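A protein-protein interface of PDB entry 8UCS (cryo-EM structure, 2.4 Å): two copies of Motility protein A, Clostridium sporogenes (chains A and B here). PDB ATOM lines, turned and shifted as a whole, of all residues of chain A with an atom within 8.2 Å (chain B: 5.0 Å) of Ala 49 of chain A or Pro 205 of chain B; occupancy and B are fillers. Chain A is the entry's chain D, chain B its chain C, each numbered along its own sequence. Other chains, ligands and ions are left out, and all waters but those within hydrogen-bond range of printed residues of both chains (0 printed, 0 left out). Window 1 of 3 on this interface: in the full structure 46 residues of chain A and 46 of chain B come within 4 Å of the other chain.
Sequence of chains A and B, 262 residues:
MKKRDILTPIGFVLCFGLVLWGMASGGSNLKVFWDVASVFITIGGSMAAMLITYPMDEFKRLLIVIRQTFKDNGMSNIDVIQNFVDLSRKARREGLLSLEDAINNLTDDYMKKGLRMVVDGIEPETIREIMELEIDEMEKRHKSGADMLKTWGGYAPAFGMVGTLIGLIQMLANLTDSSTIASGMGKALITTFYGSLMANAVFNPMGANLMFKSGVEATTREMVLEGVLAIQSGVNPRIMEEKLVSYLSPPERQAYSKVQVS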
ATOM      1  N   ILE A  41      21.782   0.437  18.585  1.00  0.00           N
ATOM      2  CA  ILE A  41      21.361  -0.416  17.479  1.00  0.00           C
ATOM      3  C   ILE A  41      22.210  -0.168  16.238  1.00  0.00           C
ATOM      4  O   ILE A  41      22.768  -1.104  15.658  1.00  0.00           O
ATOM      5  CB  ILE A  41      19.862  -0.219  17.191  1.00  0.00           C
ATOM      6  CG1 ILE A  41      19.022  -0.868  18.294  1.00  0.00           C
ATOM      7  CG2 ILE A  41      19.504  -0.804  15.837  1.00  0.00           C
ATOM      8  CD1 ILE A  41      17.595  -0.374  18.347  1.00  0.00           C
ATOM      9  N   THR A  42      22.319   1.086  15.802  1.00  0.00           N
ATOM     10  CA  THR A  42      23.027   1.343  14.552  1.00  0.00           C
ATOM     11  C   THR A  42      24.503   1.660  14.774  1.00  0.00           C
ATOM     12  O   THR A  42      25.364   1.078  14.111  1.00  0.00           O
ATOM     13  CB  THR A  42      22.342   2.470  13.761  1.00  0.00           C
ATOM     14  OG1 THR A  42      20.999   2.086  13.436  1.00  0.00           O
ATOM     15  CG2 THR A  42      23.088   2.782  12.492  1.00  0.00           C
ATOM     16  N   ILE A  43      24.820   2.575  15.690  1.00  0.00           N
ATOM     17  CA  ILE A  43      26.221   2.887  15.954  1.00  0.00           C
ATOM     18  C   ILE A  43      26.908   1.707  16.630  1.00  0.00           C
ATOM     19  O   ILE A  43      27.995   1.285  16.223  1.00  0.00           O
ATOM     20  CB  ILE A  43      26.340   4.170  16.794  1.00  0.00           C
ATOM     21  CG1 ILE A  43      25.578   5.315  16.126  1.00  0.00           C
ATOM     22  CG2 ILE A  43      27.800   4.540  16.992  1.00  0.00           C
ATOM     23  CD1 ILE A  43      25.702   6.635  16.844  1.00  0.00           C
ATOM     24  N   GLY A  44      26.284   1.160  17.673  1.00  0.00           N
ATOM     25  CA  GLY A  44      26.851  -0.004  18.332  1.00  0.00           C
ATOM     26  C   GLY A  44      26.796  -1.253  17.474  1.00  0.00           C
ATOM     27  O   GLY A  44      27.750  -2.034  17.441  1.00  0.00           O
ATOM     28  N   GLY A  45      25.679  -1.463  16.776  1.00  0.00           N
ATOM     29  CA  GLY A  45      25.531  -2.666  15.972  1.00  0.00           C
ATOM     30  C   GLY A  45      26.480  -2.720  14.790  1.00  0.00           C
ATOM     31  O   GLY A  45      27.055  -3.770  14.494  1.00  0.00           O
ATOM     32  N   SER A  46      26.648  -1.597  14.090  1.00  0.00           N
ATOM     33  CA  SER A  46      27.555  -1.578  12.948  1.00  0.00           C
ATOM     34  C   SER A  46      29.011  -1.639  13.396  1.00  0.00           C
ATOM     35  O   SER A  46      29.848  -2.246  12.720  1.00  0.00           O
ATOM     36  CB  SER A  46      27.300  -0.340  12.089  1.00  0.00           C
ATOM     37  OG  SER A  46      27.707   0.841  12.755  1.00  0.00           O
ATOM     38  N   MET A  47      29.334  -1.012  14.529  1.00  0.00           N
ATOM     39  CA  MET A  47      30.684  -1.118  15.072  1.00  0.00           C
ATOM     40  C   MET A  47      30.999  -2.549  15.487  1.00  0.00           C
ATOM     41  O   MET A  47      32.117  -3.033  15.278  1.00  0.00           O
ATOM     42  CB  MET A  47      30.855  -0.165  16.254  1.00  0.00           C
ATOM     43  CG  MET A  47      32.292   0.003  16.713  1.00  0.00           C
ATOM     44  SD  MET A  47      32.662   1.686  17.246  1.00  0.00           S
ATOM     45  CE  MET A  47      32.494   1.525  19.021  1.00  0.00           C
ATOM     46  N   ALA A  48      30.026  -3.240  16.083  1.00  0.00           N
ATOM     47  CA  ALA A  48      30.237  -4.631  16.464  1.00  0.00           C
ATOM     48  C   ALA A  48      30.343  -5.531  15.239  1.00  0.00           C
ATOM     49  O   ALA A  48      31.101  -6.508  15.244  1.00  0.00           O
ATOM     50  CB  ALA A  48      29.114  -5.096  17.385  1.00  0.00           C
ATOM     51  N   ALA A  49      29.588  -5.224  14.183  1.00  0.00           N
ATOM     52  CA  ALA A  49      29.759  -5.935  12.921  1.00  0.00           C
ATOM     53  C   ALA A  49      31.117  -5.642  12.300  1.00  0.00           C
ATOM     54  O   ALA A  49      31.678  -6.499  11.608  1.00  0.00           O
ATOM     55  CB  ALA A  49      28.637  -5.567  11.952  1.00  0.00           C
ATOM     56  N   MET A  50      31.654  -4.442  12.528  1.00  0.00           N
ATOM     57  CA  MET A  50      33.007  -4.131  12.083  1.00  0.00           C
ATOM     58  C   MET A  50      34.035  -4.986  12.815  1.00  0.00           C
ATOM     59  O   MET A  50      35.053  -5.375  12.235  1.00  0.00           O
ATOM     60  CB  MET A  50      33.298  -2.647  12.288  1.00  0.00           C
ATOM     61  CG  MET A  50      32.641  -1.736  11.272  1.00  0.00           C
ATOM     62  SD  MET A  50      33.283  -1.986   9.613  1.00  0.00           S
ATOM     63  CE  MET A  50      34.728  -0.941   9.681  1.00  0.00           C
ATOM     64  N   LEU A  51      33.786  -5.283  14.091  1.00  0.00           N
ATOM     65  CA  LEU A  51      34.688  -6.140  14.850  1.00  0.00           C
ATOM     66  C   LEU A  51      34.608  -7.595  14.410  1.00  0.00           C
ATOM     67  O   LEU A  51      35.573  -8.340  14.609  1.00  0.00           O
ATOM     68  CB  LEU A  51      34.391  -6.023  16.345  1.00  0.00           C
ATOM     69  CG  LEU A  51      34.789  -4.690  16.982  1.00  0.00           C
ATOM     70  CD1 LEU A  51      34.385  -4.642  18.445  1.00  0.00           C
ATOM     71  CD2 LEU A  51      36.280  -4.443  16.824  1.00  0.00           C
ATOM     72  N   ILE A  52      33.483  -8.020  13.831  1.00  0.00           N
ATOM     73  CA  ILE A  52      33.417  -9.347  13.230  1.00  0.00           C
ATOM     74  C   ILE A  52      34.266  -9.398  11.967  1.00  0.00           C
ATOM     75  O   ILE A  52      35.023 -10.350  11.747  1.00  0.00           O
ATOM     76  CB  ILE A  52      31.955  -9.733  12.944  1.00  0.00           C
ATOM     77  CG1 ILE A  52      31.169  -9.869  14.247  1.00  0.00           C
ATOM     78  CG2 ILE A  52      31.886 -11.024  12.136  1.00  0.00           C
ATOM     79  CD1 ILE A  52      29.706  -9.529  14.115  1.00  0.00           C
ATOM     80  N   THR A  53      34.156  -8.374  11.119  1.00  0.00           N
ATOM     81  CA  THR A  53      34.932  -8.333   9.884  1.00  0.00           C
ATOM     82  C   THR A  53      36.415  -8.143  10.168  1.00  0.00           C
ATOM     83  O   THR A  53      37.264  -8.824   9.582  1.00  0.00           O
ATOM     84  CB  THR A  53      34.421  -7.209   8.985  1.00  0.00           C
ATOM     85  OG1 THR A  53      33.036  -7.422   8.687  1.00  0.00           O
ATOM     86  CG2 THR A  53      35.215  -7.158   7.696  1.00  0.00           C
ATOM     87  N   TYR A  54      36.746  -7.217  11.062  1.00  0.00           N
ATOM     88  CA  TYR A  54      38.128  -6.854  11.342  1.00  0.00           C
ATOM     89  C   TYR A  54      38.463  -7.199  12.784  1.00  0.00           C
ATOM     90  O   TYR A  54      37.787  -6.706  13.705  1.00  0.00           O
ATOM     91  CB  TYR A  54      38.360  -5.365  11.082  1.00  0.00           C
ATOM     92  CG  TYR A  54      38.005  -4.931   9.681  1.00  0.00           C
ATOM     93  CD1 TYR A  54      38.859  -5.189   8.619  1.00  0.00           C
ATOM     94  CD2 TYR A  54      36.815  -4.265   9.420  1.00  0.00           C
ATOM     95  CE1 TYR A  54      38.541  -4.795   7.338  1.00  0.00           C
ATOM     96  CE2 TYR A  54      36.488  -3.867   8.141  1.00  0.00           C
ATOM     97  CZ  TYR A  54      37.354  -4.135   7.103  1.00  0.00           C
ATOM     98  OH  TYR A  54      37.037  -3.743   5.824  1.00  0.00           O
ATOM     99  N   PRO A  55      39.471  -8.031  13.035  1.00  0.00           N
ATOM    100  CA  PRO A  55      39.900  -8.269  14.416  1.00  0.00           C
ATOM    101  C   PRO A  55      40.369  -6.977  15.064  1.00  0.00           C
ATOM    102  O   PRO A  55      40.873  -6.070  14.398  1.00  0.00           O
ATOM    103  CB  PRO A  55      41.048  -9.277  14.271  1.00  0.00           C
ATOM    104  CG  PRO A  55      41.441  -9.231  12.830  1.00  0.00           C
ATOM    105  CD  PRO A  55      40.219  -8.848  12.066  1.00  0.00           C
ATOM    106  N   PHE A  59      41.810  -3.950  13.456  1.00  0.00           N
ATOM    107  CA  PHE A  59      40.946  -2.774  13.453  1.00  0.00           C
ATOM    108  C   PHE A  59      41.691  -1.548  13.966  1.00  0.00           C
ATOM    109  O   PHE A  59      41.555  -0.453  13.411  1.00  0.00           O
ATOM    110  CB  PHE A  59      39.699  -3.043  14.295  1.00  0.00           C
ATOM    111  CG  PHE A  59      38.613  -2.025  14.112  1.00  0.00           C
ATOM    112  CD1 PHE A  59      37.813  -2.043  12.984  1.00  0.00           C
ATOM    113  CD2 PHE A  59      38.390  -1.051  15.068  1.00  0.00           C
ATOM    114  CE1 PHE A  59      36.814  -1.109  12.813  1.00  0.00           C
ATOM    115  CE2 PHE A  59      37.390  -0.114  14.903  1.00  0.00           C
ATOM    116  CZ  PHE A  59      36.600  -0.143  13.772  1.00  0.00           C
ATOM    117  N   THR A 151      33.336  -0.325   4.195  1.00  0.00           N
ATOM    118  CA  THR A 151      32.612  -1.410   4.849  1.00  0.00           C
ATOM    119  C   THR A 151      31.714  -0.877   5.959  1.00  0.00           C
ATOM    120  O   THR A 151      30.559  -1.296   6.089  1.00  0.00           O
ATOM    121  CB  THR A 151      33.599  -2.438   5.400  1.00  0.00           C
ATOM    122  OG1 THR A 151      34.386  -2.967   4.327  1.00  0.00           O
ATOM    123  CG2 THR A 151      32.869  -3.576   6.091  1.00  0.00           C
ATOM    124  N   TRP A 152      32.228   0.054   6.764  1.00  0.00           N
ATOM    125  CA  TRP A 152      31.404   0.690   7.785  1.00  0.00           C
ATOM    126  C   TRP A 152      30.311   1.550   7.163  1.00  0.00           C
ATOM    127  O   TRP A 152      29.222   1.673   7.732  1.00  0.00           O
ATOM    128  CB  TRP A 152      32.277   1.525   8.719  1.00  0.00           C
ATOM    129  CG  TRP A 152      31.751   1.610  10.116  1.00  0.00           C
ATOM    130  CD1 TRP A 152      30.504   1.264  10.545  1.00  0.00           C
ATOM    131  CD2 TRP A 152      32.458   2.070  11.271  1.00  0.00           C
ATOM    132  NE1 TRP A 152      30.389   1.482  11.892  1.00  0.00           N
ATOM    133  CE2 TRP A 152      31.575   1.977  12.364  1.00  0.00           C
ATOM    134  CE3 TRP A 152      33.751   2.555  11.488  1.00  0.00           C
ATOM    135  CZ2 TRP A 152      31.943   2.350  13.654  1.00  0.00           C
ATOM    136  CZ3 TRP A 152      34.113   2.924  12.768  1.00  0.00           C
ATOM    137  CH2 TRP A 152      33.213   2.820  13.835  1.00  0.00           C
ATOM    138  N   TYR A 155      27.585  -0.853   6.649  1.00  0.00           N
ATOM    139  CA  TYR A 155      27.052  -1.483   7.853  1.00  0.00           C
ATOM    140  C   TYR A 155      26.096  -0.557   8.594  1.00  0.00           C
ATOM    141  O   TYR A 155      25.060  -1.004   9.096  1.00  0.00           O
ATOM    142  CB  TYR A 155      28.194  -1.909   8.776  1.00  0.00           C
ATOM    143  CG  TYR A 155      28.936  -3.150   8.337  1.00  0.00           C
ATOM    144  CD1 TYR A 155      28.620  -3.793   7.149  1.00  0.00           C
ATOM    145  CD2 TYR A 155      29.958  -3.677   9.114  1.00  0.00           C
ATOM    146  CE1 TYR A 155      29.299  -4.924   6.749  1.00  0.00           C
ATOM    147  CE2 TYR A 155      30.642  -4.806   8.723  1.00  0.00           C
ATOM    148  CZ  TYR A 155      30.308  -5.428   7.540  1.00  0.00           C
ATOM    149  OH  TYR A 155      30.989  -6.553   7.145  1.00  0.00           O
ATOM    150  N   ALA A 156      26.433   0.730   8.687  1.00  0.00           N
ATOM    151  CA  ALA A 156      25.610   1.659   9.459  1.00  0.00           C
ATOM    152  C   ALA A 156      24.203   1.824   8.894  1.00  0.00           C
ATOM    153  O   ALA A 156      23.240   1.733   9.673  1.00  0.00           O
ATOM    154  CB  ALA A 156      26.335   3.003   9.591  1.00  0.00           C
ATOM    155  N   ALA A 158      22.698  -0.369   7.095  1.00  0.00           N
ATOM    156  CA  ALA A 158      22.103  -1.694   7.240  1.00  0.00           C
ATOM    157  C   ALA A 158      21.547  -1.898   8.643  1.00  0.00           C
ATOM    158  O   ALA A 158      20.457  -2.454   8.809  1.00  0.00           O
ATOM    159  CB  ALA A 158      23.129  -2.774   6.902  1.00  0.00           C
ATOM    160  N   PHE A 159      22.284  -1.460   9.665  1.00  0.00           N
ATOM    161  CA  PHE A 159      21.786  -1.539  11.031  1.00  0.00           C
ATOM    162  C   PHE A 159      20.769  -0.453  11.345  1.00  0.00           C
ATOM    163  O   PHE A 159      19.987  -0.610  12.287  1.00  0.00           O
ATOM    164  CB  PHE A 159      22.948  -1.476  12.024  1.00  0.00           C
ATOM    165  CG  PHE A 159      23.625  -2.794  12.232  1.00  0.00           C
ATOM    166  CD1 PHE A 159      24.639  -3.206  11.384  1.00  0.00           C
ATOM    167  CD2 PHE A 159      23.234  -3.636  13.258  1.00  0.00           C
ATOM    168  CE1 PHE A 159      25.255  -4.422  11.562  1.00  0.00           C
ATOM    169  CE2 PHE A 159      23.850  -4.856  13.441  1.00  0.00           C
ATOM    170  CZ  PHE A 159      24.862  -5.249  12.591  1.00  0.00           C
ATOM    171  N   CYS B  15      27.525  -7.792  18.838  1.00  0.00           N
ATOM    172  CA  CYS B  15      26.527  -7.418  17.839  1.00  0.00           C
ATOM    173  C   CYS B  15      25.122  -7.770  18.301  1.00  0.00           C
ATOM    174  O   CYS B  15      24.228  -6.916  18.313  1.00  0.00           O
ATOM    175  CB  CYS B  15      26.841  -8.095  16.504  1.00  0.00           C
ATOM    176  SG  CYS B  15      26.167  -7.242  15.071  1.00  0.00           S
ATOM    177  N   ALA B 199      21.632 -11.465   7.948  1.00  0.00           N
ATOM    178  CA  ALA B 199      22.530 -10.979   6.906  1.00  0.00           C
ATOM    179  C   ALA B 199      23.554 -10.001   7.468  1.00  0.00           C
ATOM    180  O   ALA B 199      24.757 -10.139   7.228  1.00  0.00           O
ATOM    181  CB  ALA B 199      21.724 -10.326   5.785  1.00  0.00           C
ATOM    182  N   ASN B 200      23.095  -9.013   8.236  1.00  0.00           N
ATOM    183  CA  ASN B 200      23.944  -7.903   8.644  1.00  0.00           C
ATOM    184  C   ASN B 200      24.776  -8.193   9.883  1.00  0.00           C
ATOM    185  O   ASN B 200      25.791  -7.522  10.098  1.00  0.00           O
ATOM    186  CB  ASN B 200      23.092  -6.654   8.892  1.00  0.00           C
ATOM    187  CG  ASN B 200      22.336  -6.213   7.658  1.00  0.00           C
ATOM    188  OD1 ASN B 200      21.156  -5.877   7.727  1.00  0.00           O
ATOM    189  ND2 ASN B 200      23.013  -6.214   6.517  1.00  0.00           N
ATOM    190  N   ALA B 201      24.383  -9.166  10.700  1.00  0.00           N
ATOM    191  CA  ALA B 201      25.129  -9.470  11.912  1.00  0.00           C
ATOM    192  C   ALA B 201      25.955 -10.744  11.814  1.00  0.00           C
ATOM    193  O   ALA B 201      26.882 -10.917  12.610  1.00  0.00           O
ATOM    194  CB  ALA B 201      24.179  -9.579  13.111  1.00  0.00           C
ATOM    195  N   VAL B 202      25.647 -11.636  10.873  1.00  0.00           N
ATOM    196  CA  VAL B 202      26.349 -12.912  10.796  1.00  0.00           C
ATOM    197  C   VAL B 202      26.989 -13.115   9.428  1.00  0.00           C
ATOM    198  O   VAL B 202      28.216 -13.183   9.314  1.00  0.00           O
ATOM    199  CB  VAL B 202      25.403 -14.082  11.129  1.00  0.00           C
ATOM    200  CG1 VAL B 202      26.185 -15.378  11.246  1.00  0.00           C
ATOM    201  CG2 VAL B 202      24.637 -13.800  12.411  1.00  0.00           C
ATOM    202  N   PHE B 203      26.168 -13.189   8.378  1.00  0.00           N
ATOM    203  CA  PHE B 203      26.654 -13.689   7.094  1.00  0.00           C
ATOM    204  C   PHE B 203      27.548 -12.675   6.389  1.00  0.00           C
ATOM    205  O   PHE B 203      28.676 -12.997   6.002  1.00  0.00           O
ATOM    206  CB  PHE B 203      25.476 -14.082   6.202  1.00  0.00           C
ATOM    207  CG  PHE B 203      24.701 -15.258   6.710  1.00  0.00           C
ATOM    208  CD1 PHE B 203      25.354 -16.391   7.166  1.00  0.00           C
ATOM    209  CD2 PHE B 203      23.317 -15.233   6.737  1.00  0.00           C
ATOM    210  CE1 PHE B 203      24.642 -17.473   7.638  1.00  0.00           C
ATOM    211  CE2 PHE B 203      22.603 -16.312   7.209  1.00  0.00           C
ATOM    212  CZ  PHE B 203      23.266 -17.433   7.661  1.00  0.00           C
ATOM    213  N   ASN B 204      27.057 -11.453   6.196  1.00  0.00           N
ATOM    214  CA  ASN B 204      27.857 -10.445   5.498  1.00  0.00           C
ATOM    215  C   ASN B 204      29.139 -10.082   6.238  1.00  0.00           C
ATOM    216  O   ASN B 204      30.202 -10.047   5.595  1.00  0.00           O
ATOM    217  CB  ASN B 204      27.002  -9.206   5.212  1.00  0.00           C
ATOM    218  CG  ASN B 204      25.865  -9.490   4.252  1.00  0.00           C
ATOM    219  OD1 ASN B 204      25.858 -10.509   3.563  1.00  0.00           O
ATOM    220  ND2 ASN B 204      24.895  -8.587   4.204  1.00  0.00           N
ATOM    221  N   PRO B 205      29.131  -9.783   7.545  1.00  0.00           N
ATOM    222  CA  PRO B 205      30.412  -9.509   8.219  1.00  0.00           C
ATOM    223  C   PRO B 205      31.367 -10.691   8.225  1.00  0.00           C
ATOM    224  O   PRO B 205      32.585 -10.484   8.176  1.00  0.00           O
ATOM    225  CB  PRO B 205      29.987  -9.107   9.640  1.00  0.00           C
ATOM    226  CG  PRO B 205      28.626  -9.644   9.805  1.00  0.00           C
ATOM    227  CD  PRO B 205      27.991  -9.600   8.461  1.00  0.00           C
ATOM    228  N   MET B 206      30.860 -11.924   8.287  1.00  0.00           N
ATOM    229  CA  MET B 206      31.744 -13.084   8.226  1.00  0.00           C
ATOM    230  C   MET B 206      32.337 -13.256   6.834  1.00  0.00           C
ATOM    231  O   MET B 206      33.500 -13.650   6.694  1.00  0.00           O
ATOM    232  CB  MET B 206      30.997 -14.347   8.646  1.00  0.00           C
ATOM    233  CG  MET B 206      31.327 -14.820  10.045  1.00  0.00           C
ATOM    234  SD  MET B 206      33.000 -14.383  10.555  1.00  0.00           S
ATOM    235  CE  MET B 206      33.918 -15.814   9.991  1.00  0.00           C
ATOM    236  N   GLY B 207      31.549 -12.982   5.794  1.00  0.00           N
ATOM    237  CA  GLY B 207      32.079 -13.051   4.444  1.00  0.00           C
ATOM    238  C   GLY B 207      33.154 -12.014   4.191  1.00  0.00           C
ATOM    239  O   GLY B 207      34.166 -12.300   3.545  1.00  0.00           O
ATOM    240  N   ALA B 208      32.951 -10.796   4.693  1.00  0.00           N
ATOM    241  CA  ALA B 208      33.973  -9.764   4.567  1.00  0.00           C
ATOM    242  C   ALA B 208      35.177 -10.059   5.450  1.00  0.00           C
ATOM    243  O   ALA B 208      36.298  -9.655   5.121  1.00  0.00           O
ATOM    244  CB  ALA B 208      33.380  -8.397   4.905  1.00  0.00           C
ATOM    245  N   ASN B 209      34.965 -10.752   6.571  1.00  0.00           N
ATOM    246  CA  ASN B 209      36.082 -11.161   7.415  1.00  0.00           C
ATOM    247  C   ASN B 209      36.991 -12.143   6.687  1.00  0.00           C
ATOM    248  O   ASN B 209      38.219 -12.060   6.793  1.00  0.00           O
ATOM    249  CB  ASN B 209      35.554 -11.771   8.715  1.00  0.00           C
ATOM    250  CG  ASN B 209      36.629 -12.487   9.506  1.00  0.00           C
ATOM    251  OD1 ASN B 209      36.792 -13.699   9.397  1.00  0.00           O
ATOM    252  ND2 ASN B 209      37.367 -11.737  10.314  1.00  0.00           N
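The backbone carbonyl oxygen (O) of Ala 199 of chain B lies within hydrogen-bond range of the backbone NH (N) of Asn 204 of chain B, 2.8 Å away.
OG1 of Thr 42 of chain A sits at hydrogen-bond distance from O of Phe 159 of chain A (3.1 Å).
The side-chain hydroxyl of Thr 53 of chain A lies within hydrogen-bond range of the backbone carbonyl oxygen of Ala 49 of chain A, 3.4 Å away.
OH of Tyr 155 of chain A is in hydrogen-bond range of OG1 of Thr 53 of chain A.
No position is printed for both chains.
Of the 18 pairs that touch across the chains among the printed residues, none has its exchanged pair printed and touching as well.
Among the printed residues, pairs that only touch across the chains: Tyr 155 of chain A with Pro 205 of chain B, Phe 159 of chain A with Cys 15 of chain B, Ala 48 of chain A with Cys 15 of chain B, Ala 158 of chain A with Asn 200 of chain B, Phe 159 of chain A with Asn 200 of chain B, Ile 52 of chain A with Ala 201 of chain B, Thr 53 of chain A with Ala 208 of chain B, Ile 52 of chain A with Pro 205 of chain B, Ala 49 of chain A with Pro 205 of chain B, Tyr 155 of chain A with Ala 208 of chain B, Ile 52 of chain A with Met 206 of chain B, Tyr 155 of chain A with Asn 204 of chain B, Ala 49 of chain A with Asn 200 of chain B and Ile 52 of chain A with Cys 15 of chain B.
Of chain B, only Asn 200 and Pro 205 come within 4 Å of Ala 49 of chain A.
Pro 205 of chain B touches just these residues of chain A: Ala 49 (3.7 Å), Ile 52 (3.7 Å), Thr 53 (3.1 Å) and Tyr 155 (3.2 Å).
Of the printed residues of chain B, Thr 53 of chain A touches Pro 205 (3.1 Å), Ala 208 (3.6 Å) and Asn 209 (3.0 Å).
Of the printed residues of chain B, Ala 48 of chain A touches Cys 15.
Printed residues of chain A within 4 Å of Met 206 of chain B: Ile 52.
Printed residues of chain A within 4 Å of Cys 15 of chain B: Gly 45, Ala 48, Ile 52 and Phe 159.
The side-chain sulfur (SG) of Cys 15 of chain B lies within hydrogen-bond range of the backbone carbonyl oxygen (O) of Gly 45 of chain A, 3.6 Å away.
The backbone carbonyl oxygen (O) of Pro 205 of chain B sits at hydrogen-bond distance from the side-chain hydroxyl (OG1) of Thr 53 of chain A (3.1 Å).
ND2 of Asn 209 of chain B sits at hydrogen-bond distance from O of Ile 52 of chain A.
The side-chain amide nitrogen (ND2) of Asn 209 of chain B is in hydrogen-bond range of the backbone carbonyl oxygen (O) of Thr 53 of chain A, 3.0 Å away.
Printed residues of chain B that touch a printed residue of chain A: Cys 15, Asn 200, Ala 201, Asn 204, Pro 205, Met 206, Ala 208 and Asn 209.
Printed residues of chain A that touch a printed residue of chain B: Gly 45, Ala 48, Ala 49, Ile 52, Thr 53, Tyr 155, Ala 158 and Phe 159.
Among the printed residues, 18 pairs touch across the chains.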
